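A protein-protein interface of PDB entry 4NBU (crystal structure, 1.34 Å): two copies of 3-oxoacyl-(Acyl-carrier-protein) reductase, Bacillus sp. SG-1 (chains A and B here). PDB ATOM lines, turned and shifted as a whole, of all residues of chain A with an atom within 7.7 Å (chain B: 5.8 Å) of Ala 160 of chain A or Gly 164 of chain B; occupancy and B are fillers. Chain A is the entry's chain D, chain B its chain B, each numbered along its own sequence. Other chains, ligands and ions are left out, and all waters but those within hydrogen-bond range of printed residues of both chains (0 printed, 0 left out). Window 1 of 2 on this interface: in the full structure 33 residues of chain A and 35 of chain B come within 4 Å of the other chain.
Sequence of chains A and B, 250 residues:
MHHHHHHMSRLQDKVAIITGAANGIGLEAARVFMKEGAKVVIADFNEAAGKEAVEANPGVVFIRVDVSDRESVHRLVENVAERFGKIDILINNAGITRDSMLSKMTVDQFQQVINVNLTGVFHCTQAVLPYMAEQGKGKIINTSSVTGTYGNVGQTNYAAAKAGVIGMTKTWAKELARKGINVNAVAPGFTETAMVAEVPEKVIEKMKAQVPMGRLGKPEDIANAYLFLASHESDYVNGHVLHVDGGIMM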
ATOM      1  N   PHE A 110      14.944 -19.664 -25.203  1.00  0.00           N
ATOM      2  CA  PHE A 110      16.204 -18.985 -24.970  1.00  0.00           C
ATOM      3  C   PHE A 110      16.087 -17.518 -25.371  1.00  0.00           C
ATOM      4  O   PHE A 110      16.399 -16.618 -24.584  1.00  0.00           O
ATOM      5  CB  PHE A 110      17.324 -19.682 -25.752  1.00  0.00           C
ATOM      6  CG  PHE A 110      18.697 -19.121 -25.471  1.00  0.00           C
ATOM      7  CD1 PHE A 110      19.440 -19.586 -24.394  1.00  0.00           C
ATOM      8  CD2 PHE A 110      19.232 -18.120 -26.269  1.00  0.00           C
ATOM      9  CE1 PHE A 110      20.705 -19.069 -24.116  1.00  0.00           C
ATOM     10  CE2 PHE A 110      20.499 -17.591 -25.995  1.00  0.00           C
ATOM     11  CZ  PHE A 110      21.233 -18.071 -24.928  1.00  0.00           C
ATOM     12  N   VAL A 113      13.812 -14.926 -23.284  1.00  0.00           N
ATOM     13  CA  VAL A 113      14.396 -14.511 -22.027  1.00  0.00           C
ATOM     14  C   VAL A 113      15.554 -13.541 -22.271  1.00  0.00           C
ATOM     15  O   VAL A 113      15.703 -12.559 -21.553  1.00  0.00           O
ATOM     16  CB  VAL A 113      14.803 -15.738 -21.179  1.00  0.00           C
ATOM     17  CG1 VAL A 113      15.731 -15.353 -20.038  1.00  0.00           C
ATOM     18  CG2 VAL A 113      13.558 -16.438 -20.663  1.00  0.00           C
ATOM     19  N   ILE A 114      16.357 -13.784 -23.297  1.00  0.00           N
ATOM     20  CA  ILE A 114      17.386 -12.821 -23.679  1.00  0.00           C
ATOM     21  C   ILE A 114      16.770 -11.462 -24.052  1.00  0.00           C
ATOM     22  O   ILE A 114      17.254 -10.414 -23.607  1.00  0.00           O
ATOM     23  CB  ILE A 114      18.242 -13.345 -24.869  1.00  0.00           C
ATOM     24  CG1 ILE A 114      19.038 -14.605 -24.482  1.00  0.00           C
ATOM     25  CG2 ILE A 114      19.181 -12.251 -25.379  1.00  0.00           C
ATOM     26  CD1 ILE A 114      19.983 -14.399 -23.320  1.00  0.00           C
ATOM     27  N   ASN A 117      15.242  -9.884 -20.621  1.00  0.00           N
ATOM     28  CA  ASN A 117      16.119  -9.758 -19.472  1.00  0.00           C
ATOM     29  C   ASN A 117      17.489  -9.177 -19.777  1.00  0.00           C
ATOM     30  O   ASN A 117      18.186  -8.740 -18.860  1.00  0.00           O
ATOM     31  CB  ASN A 117      16.319 -11.107 -18.774  1.00  0.00           C
ATOM     32  CG  ASN A 117      15.051 -11.662 -18.179  1.00  0.00           C
ATOM     33  OD1 ASN A 117      13.941 -11.207 -18.486  1.00  0.00           O
ATOM     34  ND2 ASN A 117      15.197 -12.687 -17.345  1.00  0.00           N
ATOM     35  N   LEU A 118      17.895  -9.214 -21.044  1.00  0.00           N
ATOM     36  CA  LEU A 118      19.201  -8.686 -21.421  1.00  0.00           C
ATOM     37  C   LEU A 118      19.051  -7.510 -22.377  1.00  0.00           C
ATOM     38  O   LEU A 118      19.403  -6.368 -22.049  1.00  0.00           O
ATOM     39  CB  LEU A 118      20.091  -9.781 -22.017  1.00  0.00           C
ATOM     40  CG  LEU A 118      21.517  -9.333 -22.349  1.00  0.00           C
ATOM     41  CD1 LEU A 118      22.285  -8.942 -21.091  1.00  0.00           C
ATOM     42  CD2 LEU A 118      22.242 -10.424 -23.115  1.00  0.00           C
ATOM     43  N   THR A 147      21.221 -16.631  -9.823  1.00  0.00           N
ATOM     44  CA  THR A 147      21.355 -17.562 -10.941  1.00  0.00           C
ATOM     45  C   THR A 147      22.385 -17.068 -11.958  1.00  0.00           C
ATOM     46  O   THR A 147      23.116 -17.866 -12.559  1.00  0.00           O
ATOM     47  CB  THR A 147      19.984 -17.812 -11.603  1.00  0.00           C
ATOM     48  OG1 THR A 147      19.160 -18.521 -10.674  1.00  0.00           O
ATOM     49  CG2 THR A 147      20.130 -18.623 -12.884  1.00  0.00           C
ATOM     50  N   GLY A 148      22.466 -15.754 -12.133  1.00  0.00           N
ATOM     51  CA  GLY A 148      23.470 -15.151 -12.990  1.00  0.00           C
ATOM     52  C   GLY A 148      24.883 -15.319 -12.454  1.00  0.00           C
ATOM     53  O   GLY A 148      25.806 -15.560 -13.228  1.00  0.00           O
ATOM     54  N   GLY A 151      24.945 -19.742 -11.538  1.00  0.00           N
ATOM     55  CA  GLY A 151      24.288 -20.756 -12.353  1.00  0.00           C
ATOM     56  C   GLY A 151      23.156 -21.442 -11.592  1.00  0.00           C
ATOM     57  O   GLY A 151      23.104 -21.423 -10.363  1.00  0.00           O
ATOM     58  N   GLN A 155      18.050 -23.283 -15.947  1.00  0.00           N
ATOM     59  CA  GLN A 155      17.981 -21.860 -16.250  1.00  0.00           C
ATOM     60  C   GLN A 155      19.077 -21.344 -17.182  1.00  0.00           C
ATOM     61  O   GLN A 155      19.566 -20.231 -17.003  1.00  0.00           O
ATOM     62  CB  GLN A 155      17.972 -21.052 -14.944  1.00  0.00           C
ATOM     63  CG  GLN A 155      16.834 -21.449 -14.024  1.00  0.00           C
ATOM     64  CD  GLN A 155      16.464 -20.338 -13.071  1.00  0.00           C
ATOM     65  OE1 GLN A 155      17.182 -20.057 -12.109  1.00  0.00           O
ATOM     66  NE2 GLN A 155      15.350 -19.675 -13.348  1.00  0.00           N
ATOM     67  N   THR A 156      19.446 -22.130 -18.191  1.00  0.00           N
ATOM     68  CA  THR A 156      20.473 -21.702 -19.141  1.00  0.00           C
ATOM     69  C   THR A 156      20.243 -20.280 -19.634  1.00  0.00           C
ATOM     70  O   THR A 156      21.148 -19.443 -19.631  1.00  0.00           O
ATOM     71  CB  THR A 156      20.502 -22.635 -20.364  1.00  0.00           C
ATOM     72  OG1 THR A 156      21.003 -23.916 -19.971  1.00  0.00           O
ATOM     73  CG2 THR A 156      21.371 -22.057 -21.464  1.00  0.00           C
ATOM     74  N   ASN A 157      19.007 -20.012 -20.048  1.00  0.00           N
ATOM     75  CA  ASN A 157      18.667 -18.721 -20.630  1.00  0.00           C
ATOM     76  C   ASN A 157      18.673 -17.568 -19.629  1.00  0.00           C
ATOM     77  O   ASN A 157      19.226 -16.509 -19.901  1.00  0.00           O
ATOM     78  CB  ASN A 157      17.324 -18.811 -21.391  1.00  0.00           C
ATOM     79  CG  ASN A 157      16.196 -19.469 -20.570  1.00  0.00           C
ATOM     80  OD1 ASN A 157      16.385 -19.926 -19.430  1.00  0.00           O
ATOM     81  ND2 ASN A 157      15.005 -19.509 -21.160  1.00  0.00           N
ATOM     82  N   TYR A 158      18.064 -17.794 -18.475  1.00  0.00           N
ATOM     83  CA  TYR A 158      17.973 -16.785 -17.437  1.00  0.00           C
ATOM     84  C   TYR A 158      19.369 -16.494 -16.886  1.00  0.00           C
ATOM     85  O   TYR A 158      19.706 -15.336 -16.636  1.00  0.00           O
ATOM     86  CB  TYR A 158      17.055 -17.332 -16.364  1.00  0.00           C
ATOM     87  CG  TYR A 158      16.710 -16.394 -15.251  1.00  0.00           C
ATOM     88  CD1 TYR A 158      15.678 -15.478 -15.385  1.00  0.00           C
ATOM     89  CD2 TYR A 158      17.367 -16.469 -14.037  1.00  0.00           C
ATOM     90  CE1 TYR A 158      15.334 -14.633 -14.350  1.00  0.00           C
ATOM     91  CE2 TYR A 158      17.035 -15.635 -13.001  1.00  0.00           C
ATOM     92  CZ  TYR A 158      16.017 -14.719 -13.161  1.00  0.00           C
ATOM     93  OH  TYR A 158      15.676 -13.894 -12.109  1.00  0.00           O
ATOM     94  N   ALA A 159      20.190 -17.535 -16.723  1.00  0.00           N
ATOM     95  CA  ALA A 159      21.555 -17.340 -16.250  1.00  0.00           C
ATOM     96  C   ALA A 159      22.360 -16.543 -17.275  1.00  0.00           C
ATOM     97  O   ALA A 159      23.132 -15.645 -16.907  1.00  0.00           O
ATOM     98  CB  ALA A 159      22.230 -18.687 -15.969  1.00  0.00           C
ATOM     99  N   ALA A 160      22.192 -16.860 -18.558  1.00  0.00           N
ATOM    100  CA  ALA A 160      22.870 -16.097 -19.598  1.00  0.00           C
ATOM    101  C   ALA A 160      22.507 -14.626 -19.503  1.00  0.00           C
ATOM    102  O   ALA A 160      23.382 -13.758 -19.514  1.00  0.00           O
ATOM    103  CB  ALA A 160      22.514 -16.649 -20.982  1.00  0.00           C
ATOM    104  N   ALA A 161      21.207 -14.346 -19.420  1.00  0.00           N
ATOM    105  CA  ALA A 161      20.752 -12.959 -19.385  1.00  0.00           C
ATOM    106  C   ALA A 161      21.198 -12.225 -18.132  1.00  0.00           C
ATOM    107  O   ALA A 161      21.712 -11.109 -18.215  1.00  0.00           O
ATOM    108  CB  ALA A 161      19.238 -12.875 -19.520  1.00  0.00           C
ATOM    109  N   LYS A 162      21.007 -12.853 -16.976  1.00  0.00           N
ATOM    110  CA  LYS A 162      21.304 -12.194 -15.711  1.00  0.00           C
ATOM    111  C   LYS A 162      22.815 -12.011 -15.508  1.00  0.00           C
ATOM    112  O   LYS A 162      23.248 -11.007 -14.951  1.00  0.00           O
ATOM    113  CB  LYS A 162      20.652 -12.939 -14.533  1.00  0.00           C
ATOM    114  CG  LYS A 162      19.108 -12.890 -14.551  1.00  0.00           C
ATOM    115  CD  LYS A 162      18.583 -11.456 -14.604  1.00  0.00           C
ATOM    116  CE  LYS A 162      17.149 -11.395 -14.105  1.00  0.00           C
ATOM    117  NZ  LYS A 162      16.658  -9.996 -14.084  1.00  0.00           N
ATOM    118  N   ALA A 163      23.630 -12.956 -15.974  1.00  0.00           N
ATOM    119  CA  ALA A 163      25.070 -12.739 -15.954  1.00  0.00           C
ATOM    120  C   ALA A 163      25.443 -11.653 -16.953  1.00  0.00           C
ATOM    121  O   ALA A 163      26.275 -10.803 -16.656  1.00  0.00           O
ATOM    122  CB  ALA A 163      25.826 -14.032 -16.241  1.00  0.00           C
ATOM    123  N   GLY A 164      24.814 -11.654 -18.122  1.00  0.00           N
ATOM    124  CA  GLY A 164      25.076 -10.621 -19.111  1.00  0.00           C
ATOM    125  C   GLY A 164      24.794  -9.224 -18.582  1.00  0.00           C
ATOM    126  O   GLY A 164      25.508  -8.274 -18.910  1.00  0.00           O
ATOM    127  N   VAL A 165      23.748  -9.101 -17.769  1.00  0.00           N
ATOM    128  CA  VAL A 165      23.406  -7.834 -17.126  1.00  0.00           C
ATOM    129  C   VAL A 165      24.579  -7.318 -16.275  1.00  0.00           C
ATOM    130  O   VAL A 165      24.846  -6.124 -16.245  1.00  0.00           O
ATOM    131  CB  VAL A 165      22.110  -7.978 -16.284  1.00  0.00           C
ATOM    132  CG1 VAL A 165      21.960  -6.830 -15.301  1.00  0.00           C
ATOM    133  CG2 VAL A 165      20.895  -8.050 -17.203  1.00  0.00           C
ATOM    134  N   ILE A 166      25.300  -8.223 -15.628  1.00  0.00           N
ATOM    135  CA  ILE A 166      26.450  -7.831 -14.831  1.00  0.00           C
ATOM    136  C   ILE A 166      27.578  -7.323 -15.732  1.00  0.00           C
ATOM    137  O   ILE A 166      28.207  -6.308 -15.435  1.00  0.00           O
ATOM    138  CB  ILE A 166      26.909  -8.976 -13.917  1.00  0.00           C
ATOM    139  CG1 ILE A 166      25.813  -9.283 -12.898  1.00  0.00           C
ATOM    140  CG2 ILE A 166      28.220  -8.633 -13.236  1.00  0.00           C
ATOM    141  CD1 ILE A 166      26.085 -10.510 -12.050  1.00  0.00           C
ATOM    142  N   GLY A 167      27.827  -8.005 -16.848  1.00  0.00           N
ATOM    143  CA  GLY A 167      28.809  -7.510 -17.795  1.00  0.00           C
ATOM    144  C   GLY A 167      28.508  -6.098 -18.282  1.00  0.00           C
ATOM    145  O   GLY A 167      29.404  -5.254 -18.380  1.00  0.00           O
ATOM    146  N   LEU B 118      27.033 -15.379 -27.744  1.00  0.00           N
ATOM    147  CA  LEU B 118      26.225 -15.948 -26.676  1.00  0.00           C
ATOM    148  C   LEU B 118      25.326 -17.062 -27.229  1.00  0.00           C
ATOM    149  O   LEU B 118      25.468 -18.233 -26.863  1.00  0.00           O
ATOM    150  CB  LEU B 118      25.404 -14.858 -25.963  1.00  0.00           C
ATOM    151  CG  LEU B 118      24.594 -15.348 -24.770  1.00  0.00           C
ATOM    152  CD1 LEU B 118      25.530 -15.838 -23.669  1.00  0.00           C
ATOM    153  CD2 LEU B 118      23.700 -14.223 -24.242  1.00  0.00           C
ATOM    154  N   ALA B 159      30.717  -7.467 -23.650  1.00  0.00           N
ATOM    155  CA  ALA B 159      30.659  -7.759 -22.215  1.00  0.00           C
ATOM    156  C   ALA B 159      29.396  -8.527 -21.839  1.00  0.00           C
ATOM    157  O   ALA B 159      29.450  -9.477 -21.058  1.00  0.00           O
ATOM    158  CB  ALA B 159      30.762  -6.476 -21.392  1.00  0.00           C
ATOM    159  N   ALA B 160      28.248  -8.128 -22.390  1.00  0.00           N
ATOM    160  CA  ALA B 160      27.013  -8.863 -22.144  1.00  0.00           C
ATOM    161  C   ALA B 160      27.166 -10.319 -22.560  1.00  0.00           C
ATOM    162  O   ALA B 160      26.827 -11.228 -21.800  1.00  0.00           O
ATOM    163  CB  ALA B 160      25.851  -8.228 -22.898  1.00  0.00           C
ATOM    164  N   ALA B 161      27.670 -10.541 -23.772  1.00  0.00           N
ATOM    165  CA  ALA B 161      27.789 -11.896 -24.280  1.00  0.00           C
ATOM    166  C   ALA B 161      28.785 -12.722 -23.480  1.00  0.00           C
ATOM    167  O   ALA B 161      28.483 -13.849 -23.094  1.00  0.00           O
ATOM    168  CB  ALA B 161      28.166 -11.883 -25.752  1.00  0.00           C
ATOM    169  N   LYS B 162      29.955 -12.153 -23.210  1.00  0.00           N
ATOM    170  CA  LYS B 162      31.009 -12.912 -22.548  1.00  0.00           C
ATOM    171  C   LYS B 162      30.684 -13.177 -21.076  1.00  0.00           C
ATOM    172  O   LYS B 162      31.023 -14.230 -20.546  1.00  0.00           O
ATOM    173  CB  LYS B 162      32.366 -12.220 -22.721  1.00  0.00           C
ATOM    174  CG  LYS B 162      32.839 -12.173 -24.181  1.00  0.00           C
ATOM    175  CD  LYS B 162      32.973 -13.569 -24.770  1.00  0.00           C
ATOM    176  CE  LYS B 162      33.876 -13.570 -25.996  1.00  0.00           C
ATOM    177  NZ  LYS B 162      34.078 -14.947 -26.527  1.00  0.00           N
ATOM    178  N   ALA B 163      29.994 -12.248 -20.417  1.00  0.00           N
ATOM    179  CA  ALA B 163      29.519 -12.515 -19.073  1.00  0.00           C
ATOM    180  C   ALA B 163      28.422 -13.574 -19.127  1.00  0.00           C
ATOM    181  O   ALA B 163      28.395 -14.493 -18.311  1.00  0.00           O
ATOM    182  CB  ALA B 163      29.034 -11.235 -18.392  1.00  0.00           C
ATOM    183  N   GLY B 164      27.524 -13.455 -20.102  1.00  0.00           N
ATOM    184  CA  GLY B 164      26.478 -14.455 -20.290  1.00  0.00           C
ATOM    185  C   GLY B 164      27.019 -15.864 -20.465  1.00  0.00           C
ATOM    186  O   GLY B 164      26.446 -16.826 -19.944  1.00  0.00           O
ATOM    187  N   VAL B 165      28.142 -15.977 -21.164  1.00  0.00           N
ATOM    188  CA  VAL B 165      28.797 -17.268 -21.362  1.00  0.00           C
ATOM    189  C   VAL B 165      29.186 -17.897 -20.025  1.00  0.00           C
ATOM    190  O   VAL B 165      29.091 -19.108 -19.854  1.00  0.00           O
ATOM    191  CB  VAL B 165      30.014 -17.135 -22.296  1.00  0.00           C
ATOM    192  CG1 VAL B 165      30.941 -18.366 -22.220  1.00  0.00           C
ATOM    193  CG2 VAL B 165      29.549 -16.912 -23.717  1.00  0.00           C
ATOM    194  N   ILE B 166      29.585 -17.075 -19.063  1.00  0.00           N
ATOM    195  CA  ILE B 166      29.921 -17.595 -17.741  1.00  0.00           C
ATOM    196  C   ILE B 166      28.676 -18.104 -17.010  1.00  0.00           C
ATOM    197  O   ILE B 166      28.689 -19.158 -16.378  1.00  0.00           O
ATOM    198  CB  ILE B 166      30.674 -16.528 -16.915  1.00  0.00           C
ATOM    199  CG1 ILE B 166      32.009 -16.214 -17.598  1.00  0.00           C
ATOM    200  CG2 ILE B 166      30.873 -16.984 -15.477  1.00  0.00           C
ATOM    201  CD1 ILE B 166      32.802 -15.095 -16.932  1.00  0.00           C
ATOM    202  N   GLY B 167      27.580 -17.355 -17.091  1.00  0.00           N
ATOM    203  CA  GLY B 167      26.343 -17.825 -16.506  1.00  0.00           C
ATOM    204  C   GLY B 167      25.908 -19.173 -17.062  1.00  0.00           C
ATOM    205  O   GLY B 167      25.477 -20.056 -16.306  1.00  0.00           O
ATOM    206  N   MET B 168      26.035 -19.341 -18.372  1.00  0.00           N
ATOM    207  CA  MET B 168      25.697 -20.624 -18.984  1.00  0.00           C
ATOM    208  C   MET B 168      26.673 -21.712 -18.550  1.00  0.00           C
ATOM    209  O   MET B 168      26.256 -22.818 -18.225  1.00  0.00           O
ATOM    210  CB  MET B 168      25.655 -20.527 -20.512  1.00  0.00           C
ATOM    211  CG  MET B 168      24.583 -19.554 -21.006  1.00  0.00           C
ATOM    212  SD  MET B 168      24.186 -19.770 -22.750  1.00  0.00           S
ATOM    213  CE  MET B 168      25.804 -19.566 -23.498  1.00  0.00           C
ATOM    214  N   THR B 169      27.959 -21.367 -18.460  1.00  0.00           N
ATOM    215  CA  THR B 169      28.983 -22.328 -18.067  1.00  0.00           C
ATOM    216  C   THR B 169      28.677 -22.889 -16.681  1.00  0.00           C
ATOM    217  O   THR B 169      28.723 -24.100 -16.462  1.00  0.00           O
ATOM    218  CB  THR B 169      30.357 -21.655 -18.038  1.00  0.00           C
ATOM    219  OG1 THR B 169      30.721 -21.238 -19.354  1.00  0.00           O
ATOM    220  CG2 THR B 169      31.435 -22.609 -17.508  1.00  0.00           C
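Among the printed residues, pairs that only touch across the chains: Gly 164 of chain A with Ala 160 of chain B (3.3 Å), Ala 160 of chain A with Gly 164 of chain B (3.3 Å), Ala 163 of chain A with Ala 163 of chain B (3.3 Å), Gly 167 of chain A with Ala 159 of chain B (3.5 Å), Ala 159 of chain A with Gly 167 of chain B (3.5 Å), Ala 160 of chain A with Met 168 of chain B (3.6 Å), Thr 156 of chain A with Met 168 of chain B (3.7 Å), Gly 167 of chain A with Ala 163 of chain B (3.8 Å), Phe 110 of chain A with Met 168 of chain B (3.8 Å), Gly 164 of chain A with Gly 164 of chain B (3.8 Å), Ile 114 of chain A with Leu 118 of chain B (3.8 Å) and Ala 163 of chain A with Gly 167 of chain B (3.8 Å).
Ala 160 of chain A touches just these residues of chain B: Gly 164 (3.3 Å) and Met 168 (3.6 Å).
Of chain A, only Ala 160 and Gly 164 come within 4 Å of Gly 164 of chain B.
Of the printed residues of chain B, Thr 156 of chain A touches Met 168.
Of the printed residues of chain B, Gly 167 of chain A touches Ala 159 and Ala 163.
Of the printed residues of chain A, Ala 160 of chain B touches Gly 164.
Printed residues of chain B within 4 Å of Ala 159 of chain A: Gly 167 (3.5 Å).
The nearest residue of chain B that does not touch Ala 160 of chain A is Leu 118 of chain B (4.1 Å).
The nearest residue of chain A that does not touch Gly 164 of chain B is Ala 163 of chain A (4.1 Å).
Of the 21 printed residues of chain A, 8 touch a printed residue of chain B.
Printed residues of chain A that touch a printed residue of chain B: Phe 110, Ile 114, Thr 156, Ala 159, Ala 160, Ala 163, Gly 164 and Gly 167.
Hydrophobic or aromatic side chains of chain A that line the printed part of chain B: Phe 110, Ile 114, Ala 159, Ala 160 and Ala 163.
Printed residues of chain B that touch a printed residue of chain A: Leu 118, Ala 159, Ala 160, Ala 163, Gly 164, Gly 167 and Met 168.
Hydrophobic or aromatic side chains of chain B that line the printed part of chain A: Leu 118, Ala 159, Ala 163 and Met 168.
Among the printed residues, no Asp or Glu carboxylate lies within 4 Å of a Lys or Arg side-chain nitrogen of the other chain.
Ala 159 of chain A touches Gly 167 of chain B, and with the chains exchanged Gly 167 of chain A touches Ala 159 of chain B.
Ala 160 of chain A touches Gly 164 of chain B, and with the chains exchanged Gly 164 of chain A touches Ala 160 of chain B.
Ala 163 of chain B touches its own counterpart, Ala 163 of chain A.
Ala 163 of chain A touches Gly 167 of chain B, and with the chains exchanged Gly 167 of chain A touches Ala 163 of chain B.
Positions printed for both chains: 118, 159, 160, 161, 162, 163, 164, 165, 166 and 167.
Of the 12 pairs that touch across the chains among the printed residues, 8 have their exchanged pair printed and touching as well.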
